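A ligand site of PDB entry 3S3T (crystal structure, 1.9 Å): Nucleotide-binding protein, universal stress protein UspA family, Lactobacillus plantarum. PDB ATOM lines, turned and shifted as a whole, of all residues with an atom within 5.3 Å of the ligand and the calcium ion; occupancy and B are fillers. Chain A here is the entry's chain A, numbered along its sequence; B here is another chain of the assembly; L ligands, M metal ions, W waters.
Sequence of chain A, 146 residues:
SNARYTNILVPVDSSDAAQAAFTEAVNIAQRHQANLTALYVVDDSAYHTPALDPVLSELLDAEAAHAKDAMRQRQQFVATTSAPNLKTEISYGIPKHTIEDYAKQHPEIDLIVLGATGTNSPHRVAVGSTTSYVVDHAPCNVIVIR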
ATOM      1  N   PRO A  11      31.429  34.018   2.627  1.00  0.00           N
ATOM      2  CA  PRO A  11      31.003  33.049   3.621  1.00  0.00           C
ATOM      3  C   PRO A  11      30.923  31.667   2.972  1.00  0.00           C
ATOM      4  O   PRO A  11      30.311  31.520   1.900  1.00  0.00           O
ATOM      5  CB  PRO A  11      29.641  33.584   4.090  1.00  0.00           C
ATOM      6  CG  PRO A  11      29.611  35.014   3.669  1.00  0.00           C
ATOM      7  CD  PRO A  11      30.383  35.009   2.366  1.00  0.00           C
ATOM      8  N   VAL A  12      31.530  30.662   3.607  1.00  0.00           N
ATOM      9  CA  VAL A  12      31.384  29.298   3.125  1.00  0.00           C
ATOM     10  C   VAL A  12      30.825  28.340   4.187  1.00  0.00           C
ATOM     11  O   VAL A  12      31.188  28.423   5.359  1.00  0.00           O
ATOM     12  CB  VAL A  12      32.753  28.725   2.672  1.00  0.00           C
ATOM     13  CG1 VAL A  12      33.228  29.407   1.404  1.00  0.00           C
ATOM     14  CG2 VAL A  12      33.772  28.894   3.789  1.00  0.00           C
ATOM     15  N   ASP A  13      29.988  27.399   3.749  1.00  0.00           N
ATOM     16  CA  ASP A  13      29.699  26.186   4.545  1.00  0.00           C
ATOM     17  C   ASP A  13      30.548  25.090   3.940  1.00  0.00           C
ATOM     18  O   ASP A  13      31.567  25.378   3.270  1.00  0.00           O
ATOM     19  CB  ASP A  13      28.202  25.848   4.589  1.00  0.00           C
ATOM     20  CG  ASP A  13      27.611  25.636   3.215  1.00  0.00           C
ATOM     21  OD1 ASP A  13      28.392  25.389   2.288  1.00  0.00           O
ATOM     22  OD2 ASP A  13      26.392  25.677   3.080  1.00  0.00           O
ATOM     23  N   SER A  15      29.628  22.900   1.711  1.00  0.00           N
ATOM     24  CA  SER A  15      29.071  22.400   0.458  1.00  0.00           C
ATOM     25  C   SER A  15      29.970  22.656  -0.739  1.00  0.00           C
ATOM     26  O   SER A  15      30.797  23.584  -0.730  1.00  0.00           O
ATOM     27  CB  SER A  15      27.709  23.027   0.224  1.00  0.00           C
ATOM     28  OG  SER A  15      27.865  24.424   0.006  1.00  0.00           O
ATOM     29  N   ALA A  17      28.787  23.925  -3.415  1.00  0.00           N
ATOM     30  CA  ALA A  17      28.277  25.168  -3.961  1.00  0.00           C
ATOM     31  C   ALA A  17      29.024  26.336  -3.335  1.00  0.00           C
ATOM     32  O   ALA A  17      29.350  27.280  -4.032  1.00  0.00           O
ATOM     33  CB  ALA A  17      26.743  25.318  -3.740  1.00  0.00           C
ATOM     34  N   ALA A  18      29.279  26.258  -2.025  1.00  0.00           N
ATOM     35  CA  ALA A  18      30.042  27.295  -1.323  1.00  0.00           C
ATOM     36  C   ALA A  18      31.488  27.326  -1.757  1.00  0.00           C
ATOM     37  O   ALA A  18      32.108  28.397  -1.830  1.00  0.00           O
ATOM     38  CB  ALA A  18      29.940  27.104   0.179  1.00  0.00           C
ATOM     39  N   ALA A  21      31.682  29.145  -4.939  1.00  0.00           N
ATOM     40  CA  ALA A  21      31.652  30.567  -4.534  1.00  0.00           C
ATOM     41  C   ALA A  21      33.034  31.092  -4.135  1.00  0.00           C
ATOM     42  O   ALA A  21      33.452  32.158  -4.542  1.00  0.00           O
ATOM     43  CB  ALA A  21      30.651  30.736  -3.336  1.00  0.00           C
ATOM     44  N   LEU A  39      34.841  33.065   5.500  1.00  0.00           N
ATOM     45  CA  LEU A  39      34.212  32.960   6.819  1.00  0.00           C
ATOM     46  C   LEU A  39      33.347  31.712   6.884  1.00  0.00           C
ATOM     47  O   LEU A  39      32.414  31.588   6.111  1.00  0.00           O
ATOM     48  CB  LEU A  39      33.340  34.185   7.099  1.00  0.00           C
ATOM     49  CG  LEU A  39      32.366  34.148   8.291  1.00  0.00           C
ATOM     50  CD1 LEU A  39      33.124  34.017   9.706  1.00  0.00           C
ATOM     51  CD2 LEU A  39      31.520  35.361   8.261  1.00  0.00           C
ATOM     52  N   TYR A  40      33.673  30.776   7.770  1.00  0.00           N
ATOM     53  CA  TYR A  40      32.783  29.647   8.078  1.00  0.00           C
ATOM     54  C   TYR A  40      32.107  29.871   9.415  1.00  0.00           C
ATOM     55  O   TYR A  40      32.777  30.080  10.436  1.00  0.00           O
ATOM     56  CB  TYR A  40      33.597  28.343   8.127  1.00  0.00           C
ATOM     57  CG  TYR A  40      32.775  27.073   8.292  1.00  0.00           C
ATOM     58  CD1 TYR A  40      32.198  26.724   9.517  1.00  0.00           C
ATOM     59  CD2 TYR A  40      32.606  26.196   7.214  1.00  0.00           C
ATOM     60  CE1 TYR A  40      31.423  25.568   9.636  1.00  0.00           C
ATOM     61  CE2 TYR A  40      31.872  25.003   7.354  1.00  0.00           C
ATOM     62  CZ  TYR A  40      31.286  24.706   8.529  1.00  0.00           C
ATOM     63  OH  TYR A  40      30.582  23.545   8.605  1.00  0.00           O
ATOM     64  N   VAL A  41      30.780  29.808   9.439  1.00  0.00           N
ATOM     65  CA  VAL A  41      30.063  29.931  10.701  1.00  0.00           C
ATOM     66  C   VAL A  41      29.585  28.578  11.226  1.00  0.00           C
ATOM     67  O   VAL A  41      28.810  27.877  10.582  1.00  0.00           O
ATOM     68  CB  VAL A  41      28.872  30.894  10.614  1.00  0.00           C
ATOM     69  CG1 VAL A  41      28.310  31.182  12.051  1.00  0.00           C
ATOM     70  CG2 VAL A  41      29.306  32.216   9.988  1.00  0.00           C
ATOM     71  N   VAL A  42      30.056  28.234  12.434  1.00  0.00           N
ATOM     72  CA  VAL A  42      29.614  27.018  13.133  1.00  0.00           C
ATOM     73  C   VAL A  42      28.266  27.327  13.812  1.00  0.00           C
ATOM     74  O   VAL A  42      28.187  28.115  14.769  1.00  0.00           O
ATOM     75  CB  VAL A  42      30.635  26.572  14.201  1.00  0.00           C
ATOM     76  CG1 VAL A  42      30.149  25.334  14.912  1.00  0.00           C
ATOM     77  CG2 VAL A  42      32.023  26.358  13.630  1.00  0.00           C
ATOM     78  N   PRO A  95      24.224  31.317  11.397  1.00  0.00           N
ATOM     79  CA  PRO A  95      25.022  31.717  10.237  1.00  0.00           C
ATOM     80  C   PRO A  95      24.635  33.013   9.518  1.00  0.00           C
ATOM     81  O   PRO A  95      25.494  33.880   9.298  1.00  0.00           O
ATOM     82  CB  PRO A  95      24.889  30.508   9.336  1.00  0.00           C
ATOM     83  CG  PRO A  95      24.984  29.377  10.322  1.00  0.00           C
ATOM     84  CD  PRO A  95      24.088  29.844  11.446  1.00  0.00           C
ATOM     85  N   ILE A  99      26.984  36.485   9.394  1.00  0.00           N
ATOM     86  CA  ILE A  99      27.463  37.010   8.130  1.00  0.00           C
ATOM     87  C   ILE A  99      27.060  38.489   8.015  1.00  0.00           C
ATOM     88  O   ILE A  99      27.888  39.358   7.735  1.00  0.00           O
ATOM     89  CB  ILE A  99      26.898  36.184   6.921  1.00  0.00           C
ATOM     90  CG1 ILE A  99      27.553  34.780   6.871  1.00  0.00           C
ATOM     91  CG2 ILE A  99      27.133  36.952   5.612  1.00  0.00           C
ATOM     92  CD1 ILE A  99      26.789  33.758   6.012  1.00  0.00           C
ATOM     93  N   VAL A 113      30.330  37.370  -1.413  1.00  0.00           N
ATOM     94  CA  VAL A 113      30.189  36.351  -2.432  1.00  0.00           C
ATOM     95  C   VAL A 113      29.557  35.109  -1.783  1.00  0.00           C
ATOM     96  O   VAL A 113      30.034  34.624  -0.782  1.00  0.00           O
ATOM     97  CB  VAL A 113      31.559  36.021  -3.089  1.00  0.00           C
ATOM     98  CG1 VAL A 113      31.410  34.924  -4.122  1.00  0.00           C
ATOM     99  CG2 VAL A 113      32.206  37.306  -3.708  1.00  0.00           C
ATOM    100  N   LEU A 114      28.477  34.609  -2.357  1.00  0.00           N
ATOM    101  CA  LEU A 114      27.711  33.473  -1.764  1.00  0.00           C
ATOM    102  C   LEU A 114      27.411  32.423  -2.795  1.00  0.00           C
ATOM    103  O   LEU A 114      27.139  32.730  -3.970  1.00  0.00           O
ATOM    104  CB  LEU A 114      26.346  33.968  -1.207  1.00  0.00           C
ATOM    105  CG  LEU A 114      26.391  34.885   0.021  1.00  0.00           C
ATOM    106  CD1 LEU A 114      25.074  35.673   0.142  1.00  0.00           C
ATOM    107  CD2 LEU A 114      26.720  34.141   1.342  1.00  0.00           C
ATOM    108  N   GLY A 115      27.365  31.159  -2.379  1.00  0.00           N
ATOM    109  CA  GLY A 115      26.777  30.132  -3.229  1.00  0.00           C
ATOM    110  C   GLY A 115      25.285  30.318  -3.244  1.00  0.00           C
ATOM    111  O   GLY A 115      24.682  30.747  -2.275  1.00  0.00           O
ATOM    112  N   ALA A 116      24.633  29.943  -4.334  1.00  0.00           N
ATOM    113  CA  ALA A 116      23.167  29.991  -4.335  1.00  0.00           C
ATOM    114  C   ALA A 116      22.520  29.057  -3.284  1.00  0.00           C
ATOM    115  O   ALA A 116      21.559  29.447  -2.615  1.00  0.00           O
ATOM    116  CB  ALA A 116      22.661  29.657  -5.709  1.00  0.00           C
ATOM    117  N   THR A 117      23.058  27.847  -3.160  1.00  0.00           N
ATOM    118  CA  THR A 117      22.529  26.843  -2.240  1.00  0.00           C
ATOM    119  C   THR A 117      23.705  26.354  -1.406  1.00  0.00           C
ATOM    120  O   THR A 117      24.855  26.807  -1.611  1.00  0.00           O
ATOM    121  CB  THR A 117      21.880  25.678  -2.973  1.00  0.00           C
ATOM    122  OG1 THR A 117      22.820  25.093  -3.873  1.00  0.00           O
ATOM    123  CG2 THR A 117      20.689  26.154  -3.791  1.00  0.00           C
ATOM    124  N   GLY A 118      23.418  25.524  -0.423  1.00  0.00           N
ATOM    125  CA  GLY A 118      24.415  25.053   0.545  1.00  0.00           C
ATOM    126  C   GLY A 118      24.222  23.579   0.878  1.00  0.00           C
ATOM    127  O   GLY A 118      23.882  22.815  -0.019  1.00  0.00           O
ATOM    128  N   THR A 119      24.358  23.188   2.133  1.00  0.00           N
ATOM    129  CA  THR A 119      24.335  21.758   2.472  1.00  0.00           C
ATOM    130  C   THR A 119      22.908  21.173   2.552  1.00  0.00           C
ATOM    131  O   THR A 119      22.748  19.973   2.375  1.00  0.00           O
ATOM    132  CB  THR A 119      25.056  21.450   3.792  1.00  0.00           C
ATOM    133  OG1 THR A 119      24.362  22.060   4.870  1.00  0.00           O
ATOM    134  CG2 THR A 119      26.491  21.914   3.795  1.00  0.00           C
ATOM    135  N   ASN A 120      21.873  21.992   2.823  1.00  0.00           N
ATOM    136  CA  ASN A 120      20.537  21.407   3.105  1.00  0.00           C
ATOM    137  C   ASN A 120      19.537  21.336   1.963  1.00  0.00           C
ATOM    138  O   ASN A 120      18.751  20.395   1.930  1.00  0.00           O
ATOM    139  CB  ASN A 120      19.828  22.104   4.286  1.00  0.00           C
ATOM    140  CG  ASN A 120      20.365  21.660   5.662  1.00  0.00           C
ATOM    141  OD1 ASN A 120      21.313  20.901   5.783  1.00  0.00           O
ATOM    142  ND2 ASN A 120      19.718  22.163   6.709  1.00  0.00           N
ATOM    143  N   SER A 121      19.496  22.306   1.051  1.00  0.00           N
ATOM    144  CA  SER A 121      18.277  22.440   0.211  1.00  0.00           C
ATOM    145  C   SER A 121      18.409  22.477  -1.320  1.00  0.00           C
ATOM    146  O   SER A 121      17.463  22.904  -2.017  1.00  0.00           O
ATOM    147  CB  SER A 121      17.460  23.673   0.685  1.00  0.00           C
ATOM    148  OG  SER A 121      16.979  23.533   2.022  1.00  0.00           O
ATOM    149  N   PRO A 122      19.529  21.998  -1.876  1.00  0.00           N
ATOM    150  CA  PRO A 122      19.581  22.000  -3.335  1.00  0.00           C
ATOM    151  C   PRO A 122      18.454  21.249  -4.042  1.00  0.00           C
ATOM    152  O   PRO A 122      18.122  21.588  -5.169  1.00  0.00           O
ATOM    153  CB  PRO A 122      20.934  21.341  -3.639  1.00  0.00           C
ATOM    154  CG  PRO A 122      21.385  20.741  -2.394  1.00  0.00           C
ATOM    155  CD  PRO A 122      20.767  21.499  -1.280  1.00  0.00           C
ATOM    156  N   VAL A 125      15.068  24.071  -3.372  1.00  0.00           N
ATOM    157  CA  VAL A 125      15.072  25.507  -3.699  1.00  0.00           C
ATOM    158  C   VAL A 125      16.212  25.840  -4.655  1.00  0.00           C
ATOM    159  O   VAL A 125      17.224  25.120  -4.671  1.00  0.00           O
ATOM    160  CB  VAL A 125      15.295  26.349  -2.436  1.00  0.00           C
ATOM    161  CG1 VAL A 125      14.222  26.067  -1.369  1.00  0.00           C
ATOM    162  CG2 VAL A 125      16.686  26.105  -1.879  1.00  0.00           C
ATOM    163  N   GLY A 128      19.009  29.265  -1.354  1.00  0.00           N
ATOM    164  CA  GLY A 128      18.896  28.980   0.055  1.00  0.00           C
ATOM    165  C   GLY A 128      18.567  30.166   0.951  1.00  0.00           C
ATOM    166  O   GLY A 128      18.715  31.346   0.542  1.00  0.00           O
ATOM    167  N   SER A 129      18.138  29.850   2.159  1.00  0.00           N
ATOM    168  CA  SER A 129      17.614  30.868   3.060  1.00  0.00           C
ATOM    169  C   SER A 129      18.765  31.720   3.632  1.00  0.00           C
ATOM    170  O   SER A 129      18.560  32.879   3.887  1.00  0.00           O
ATOM    171  CB  SER A 129      16.761  30.250   4.173  1.00  0.00           C
ATOM    172  OG  SER A 129      17.512  29.449   5.045  1.00  0.00           O
ATOM    173  N   THR A 130      19.962  31.172   3.774  1.00  0.00           N
ATOM    174  CA  THR A 130      21.128  31.994   4.197  1.00  0.00           C
ATOM    175  C   THR A 130      21.410  33.053   3.132  1.00  0.00           C
ATOM    176  O   THR A 130      21.518  34.238   3.451  1.00  0.00           O
ATOM    177  CB  THR A 130      22.409  31.182   4.506  1.00  0.00           C
ATOM    178  OG1 THR A 130      22.117  30.139   5.433  1.00  0.00           O
ATOM    179  CG2 THR A 130      23.514  32.079   5.111  1.00  0.00           C
ATOM    180  N   THR A 131      21.463  32.641   1.868  1.00  0.00           N
ATOM    181  CA  THR A 131      21.719  33.528   0.780  1.00  0.00           C
ATOM    182  C   THR A 131      20.622  34.574   0.626  1.00  0.00           C
ATOM    183  O   THR A 131      20.950  35.781   0.530  1.00  0.00           O
ATOM    184  CB  THR A 131      21.954  32.802  -0.547  1.00  0.00           C
ATOM    185  OG1 THR A 131      23.169  32.061  -0.450  1.00  0.00           O
ATOM    186  CG2 THR A 131      22.092  33.773  -1.728  1.00  0.00           C
ATOM    187  N   ILE B  94      14.929  17.829   8.022  1.00  0.00           N
ATOM    188  CA  ILE B  94      15.074  19.265   7.866  1.00  0.00           C
ATOM    189  C   ILE B  94      13.662  19.847   8.086  1.00  0.00           C
ATOM    190  O   ILE B  94      12.771  19.515   7.325  1.00  0.00           O
ATOM    191  CB  ILE B  94      15.656  19.626   6.454  1.00  0.00           C
ATOM    192  CG1 ILE B  94      17.113  19.193   6.332  1.00  0.00           C
ATOM    193  CG2 ILE B  94      15.578  21.152   6.242  1.00  0.00           C
ATOM    194  CD1 ILE B  94      17.617  19.018   4.921  1.00  0.00           C
ATOM    195  N   LYS B  96      11.628  22.529   7.496  1.00  0.00           N
ATOM    196  CA  LYS B  96      10.746  23.058   6.462  1.00  0.00           C
ATOM    197  C   LYS B  96      10.369  22.012   5.415  1.00  0.00           C
ATOM    198  O   LYS B  96       9.209  21.956   4.975  1.00  0.00           O
ATOM    199  CB  LYS B  96      11.287  24.309   5.845  1.00  0.00           C
ATOM    200  CG  LYS B  96      12.501  24.215   4.997  1.00  0.00           C
ATOM    201  CD  LYS B  96      13.144  25.616   4.943  1.00  0.00           C
ATOM    202  CE  LYS B  96      14.456  25.589   4.176  1.00  0.00           C
ATOM    203  NZ  LYS B  96      15.206  26.940   4.187  1.00  0.00           N
ATOM    204  N   HIS B  97      11.331  21.164   5.053  1.00  0.00           N
ATOM    205  CA  HIS B  97      11.057  20.053   4.115  1.00  0.00           C
ATOM    206  C   HIS B  97      10.065  19.039   4.728  1.00  0.00           C
ATOM    207  O   HIS B  97       9.210  18.532   4.064  1.00  0.00           O
ATOM    208  CB  HIS B  97      12.304  19.272   3.792  1.00  0.00           C
ATOM    209  CG  HIS B  97      13.420  20.077   3.220  1.00  0.00           C
ATOM    210  ND1 HIS B  97      14.701  19.576   3.102  1.00  0.00           N
ATOM    211  CD2 HIS B  97      13.464  21.339   2.737  1.00  0.00           C
ATOM    212  CE1 HIS B  97      15.492  20.509   2.579  1.00  0.00           C
ATOM    213  NE2 HIS B  97      14.757  21.570   2.327  1.00  0.00           N
HETATM  214  P1  LIG L   1      18.695  26.262   3.657  1.00  0.00           P
HETATM  215  O1  LIG L   1      19.701  26.414   4.768  1.00  0.00           O
HETATM  216  O2  LIG L   1      17.865  25.017   3.795  1.00  0.00           O
HETATM  217  O3  LIG L   1      17.777  27.446   3.413  1.00  0.00           O
HETATM  218  P2  LIG L   1      20.949  25.554   1.924  1.00  0.00           P
HETATM  219  O4  LIG L   1      20.906  24.692   0.696  1.00  0.00           O
HETATM  220  O5  LIG L   1      21.670  25.044   3.124  1.00  0.00           O
HETATM  221  O6  LIG L   1      19.444  25.966   2.257  1.00  0.00           O
HETATM  222  P3  LIG L   1      22.167  28.169   2.277  1.00  0.00           P
HETATM  223  O7  LIG L   1      22.331  27.842   3.734  1.00  0.00           O
HETATM  224  O8  LIG L   1      21.403  29.396   1.996  1.00  0.00           O
HETATM  225  O9  LIG L   1      21.561  26.977   1.431  1.00  0.00           O
HETATM  226  O10 LIG L   1      23.689  28.315   1.690  1.00  0.00           O
HETATM  227  C1  LIG L   1      23.937  29.198   0.598  1.00  0.00           C
HETATM  228  C2  LIG L   1      25.328  29.828   0.722  1.00  0.00           C
HETATM  229  O11 LIG L   1      25.315  30.497   1.981  1.00  0.00           O
HETATM  230  C3  LIG L   1      26.452  28.822   0.810  1.00  0.00           C
HETATM  231  O12 LIG L   1      26.902  28.387  -0.469  1.00  0.00           O
HETATM  232  C4  LIG L   1      27.451  29.632   1.608  1.00  0.00           C
HETATM  233  O13 LIG L   1      28.064  30.537   0.697  1.00  0.00           O
HETATM  234  C5  LIG L   1      26.589  30.407   2.601  1.00  0.00           C
HETATM  235  N1  LIG L   1      26.499  29.724   3.881  1.00  0.00           N
HETATM  236  C6  LIG L   1      25.548  28.827   4.290  1.00  0.00           C
HETATM  237  N2  LIG L   1      25.805  28.378   5.539  1.00  0.00           N
HETATM  238  C7  LIG L   1      26.926  28.998   5.931  1.00  0.00           C
HETATM  239  C8  LIG L   1      27.759  28.949   7.125  1.00  0.00           C
HETATM  240  N3  LIG L   1      27.383  28.150   8.142  1.00  0.00           N
HETATM  241  N4  LIG L   1      28.890  29.736   7.164  1.00  0.00           N
HETATM  242  C9  LIG L   1      29.216  30.515   6.123  1.00  0.00           C
HETATM  243  N5  LIG L   1      28.523  30.583   4.964  1.00  0.00           N
HETATM  244  C10 LIG L   1      27.393  29.858   4.847  1.00  0.00           C
HETATM  245 CA    CA M   1      22.097  26.029   4.966  1.00  0.00          CA
HETATM  246  O   HOH W   1      22.209  24.067   6.047  1.00  0.00           O
HETATM  247  O   HOH W   2      17.279  24.079   6.272  1.00  0.00           O
HETATM  248  O   HOH W   3      25.614  25.938   8.819  1.00  0.00           O
HETATM  249  O   HOH W   4      23.474  27.226   6.628  1.00  0.00           O
HETATM  250  O   HOH W   5      24.360  25.310   4.767  1.00  0.00           O
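No residue comes within 4 Å of the calcium ion.
The nearest printed residue that does not touch the calcium ion is Thr 130 (4.1 Å).
Water W1 lies within hydrogen-bond range of OG1 of Thr 119 (3.2 Å) and ND2 of Asn 120 (3.2 Å).
Water W4 bridges a nitrogen (N2) of the ligand (2.8 Å) and the side-chain hydroxyl of Thr 130 (3.4 Å).
Water W5 lies within hydrogen-bond range of the side-chain carboxylate (OD2) of Asp 13 (2.7 Å), the side-chain hydroxyl (OG1) of Thr 119 (3.3 Å) and a nitrogen (N2) of the ligand (3.5 Å).
Water W2 bridges an oxygen (O2) of the ligand (2.7 Å) and the side-chain amide nitrogen of Asn 120 (3.1 Å).
The side-chain hydroxyl of Ser 129 lies within hydrogen-bond range of an oxygen (O3) of the ligand (2.6 Å).
The backbone carbonyl oxygen (O) of Val 41 sits at hydrogen-bond distance from a nitrogen (N3) of the ligand (2.8 Å).
An oxygen (O12) of the ligand sits at hydrogen-bond distance from the backbone carbonyl oxygen of Thr 117 (2.8 Å).
The backbone NH (N) of Gly 115 sits at hydrogen-bond distance from an oxygen (O13) of the ligand, 3.2 Å away.
The backbone NH (N) of Ser 129 is in hydrogen-bond range of an oxygen (O3) of the ligand (2.7 Å).
The side-chain hydroxyl (OG1) of Thr 130 sits close to an oxygen (O7) of the ligand (2.9 Å).
N of Thr 119 sits close to O5 of the ligand (3.4 Å).
An oxygen (O8) of the ligand lies within hydrogen-bond range of the backbone NH of Thr 131 (3.2 Å).
An oxygen (O4) of the ligand sits at hydrogen-bond distance from the backbone NH of Gly 118, at 2.9 Å.
The backbone NH (N) of Thr 130 lies within hydrogen-bond range of an oxygen (O8) of the ligand (2.9 Å).
The backbone NH (N) of Val 12 lies within hydrogen-bond range of a nitrogen (N5) of the ligand, at 3.3 Å.
The backbone carbonyl oxygen (O) of Pro 11 sits at hydrogen-bond distance from an oxygen (O13) of the ligand.
An oxygen (O4) of the ligand lies within hydrogen-bond range of the backbone NH (N) of Ser 121, 2.8 Å away.
The backbone NH (N) of Asn 120 lies close to an oxygen (O5) of the ligand, 3.1 Å away.
A nitrogen (N4) of the ligand is in hydrogen-bond range of the backbone NH (N) of Val 41 (3.0 Å).
The side-chain hydroxyl of Ser 121 lies within hydrogen-bond range of an oxygen (O2) of the ligand (2.5 Å).
The side-chain amino group (NZ) of Lys 96 of chain B is in salt-bridge range of an oxygen (O3) of the ligand, 2.7 Å away.
Merely in contact with the ligand: Asp 13 (3.5 Å), Ala 18 (3.4 Å), Leu 39 (3.4 Å), Tyr 40 (3.9 Å), Pro 95 (3.5 Å), Ile 99 (3.8 Å), Leu 114 (3.8 Å), Pro 122 (3.8 Å) and Gly 128 (3.1 Å).
The nearest printed residue that does not touch the ligand is Ala 116 (4.01 Å).
The side-chain hydroxyl of Ser 15 lies within hydrogen-bond range of the side-chain carboxylate of Asp 13, at 2.5 Å.
O of Ala 116 is in hydrogen-bond range of N of Gly 128, 2.9 Å away.
The backbone NH of Val 12 is in hydrogen-bond range of the backbone carbonyl oxygen of Leu 39 (2.8 Å).
A ring nitrogen (NE2) of His 97 of chain B sits at hydrogen-bond distance from the side-chain hydroxyl of Ser 121 (3.0 Å).
The backbone carbonyl oxygen (O) of Gly 115 is in hydrogen-bond range of the side-chain hydroxyl (OG1) of Thr 131, 2.7 Å away.
The backbone NH (N) of Thr 119 is in hydrogen-bond range of the side-chain carboxylate (OD2) of Asp 13, 3.4 Å away.
The side-chain hydroxyl (OG1) of Thr 119 is in hydrogen-bond range of the side-chain amide oxygen (OD1) of Asn 120.
N of Ala 18 sits at hydrogen-bond distance from OG of Ser 15 (3.1 Å).
The calcium ion is bound by O5 of the ligand, O7 of the ligand, water W1, water W5, O1 of the ligand and water W4.
The calcium ion has six donor atoms within binding distance.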
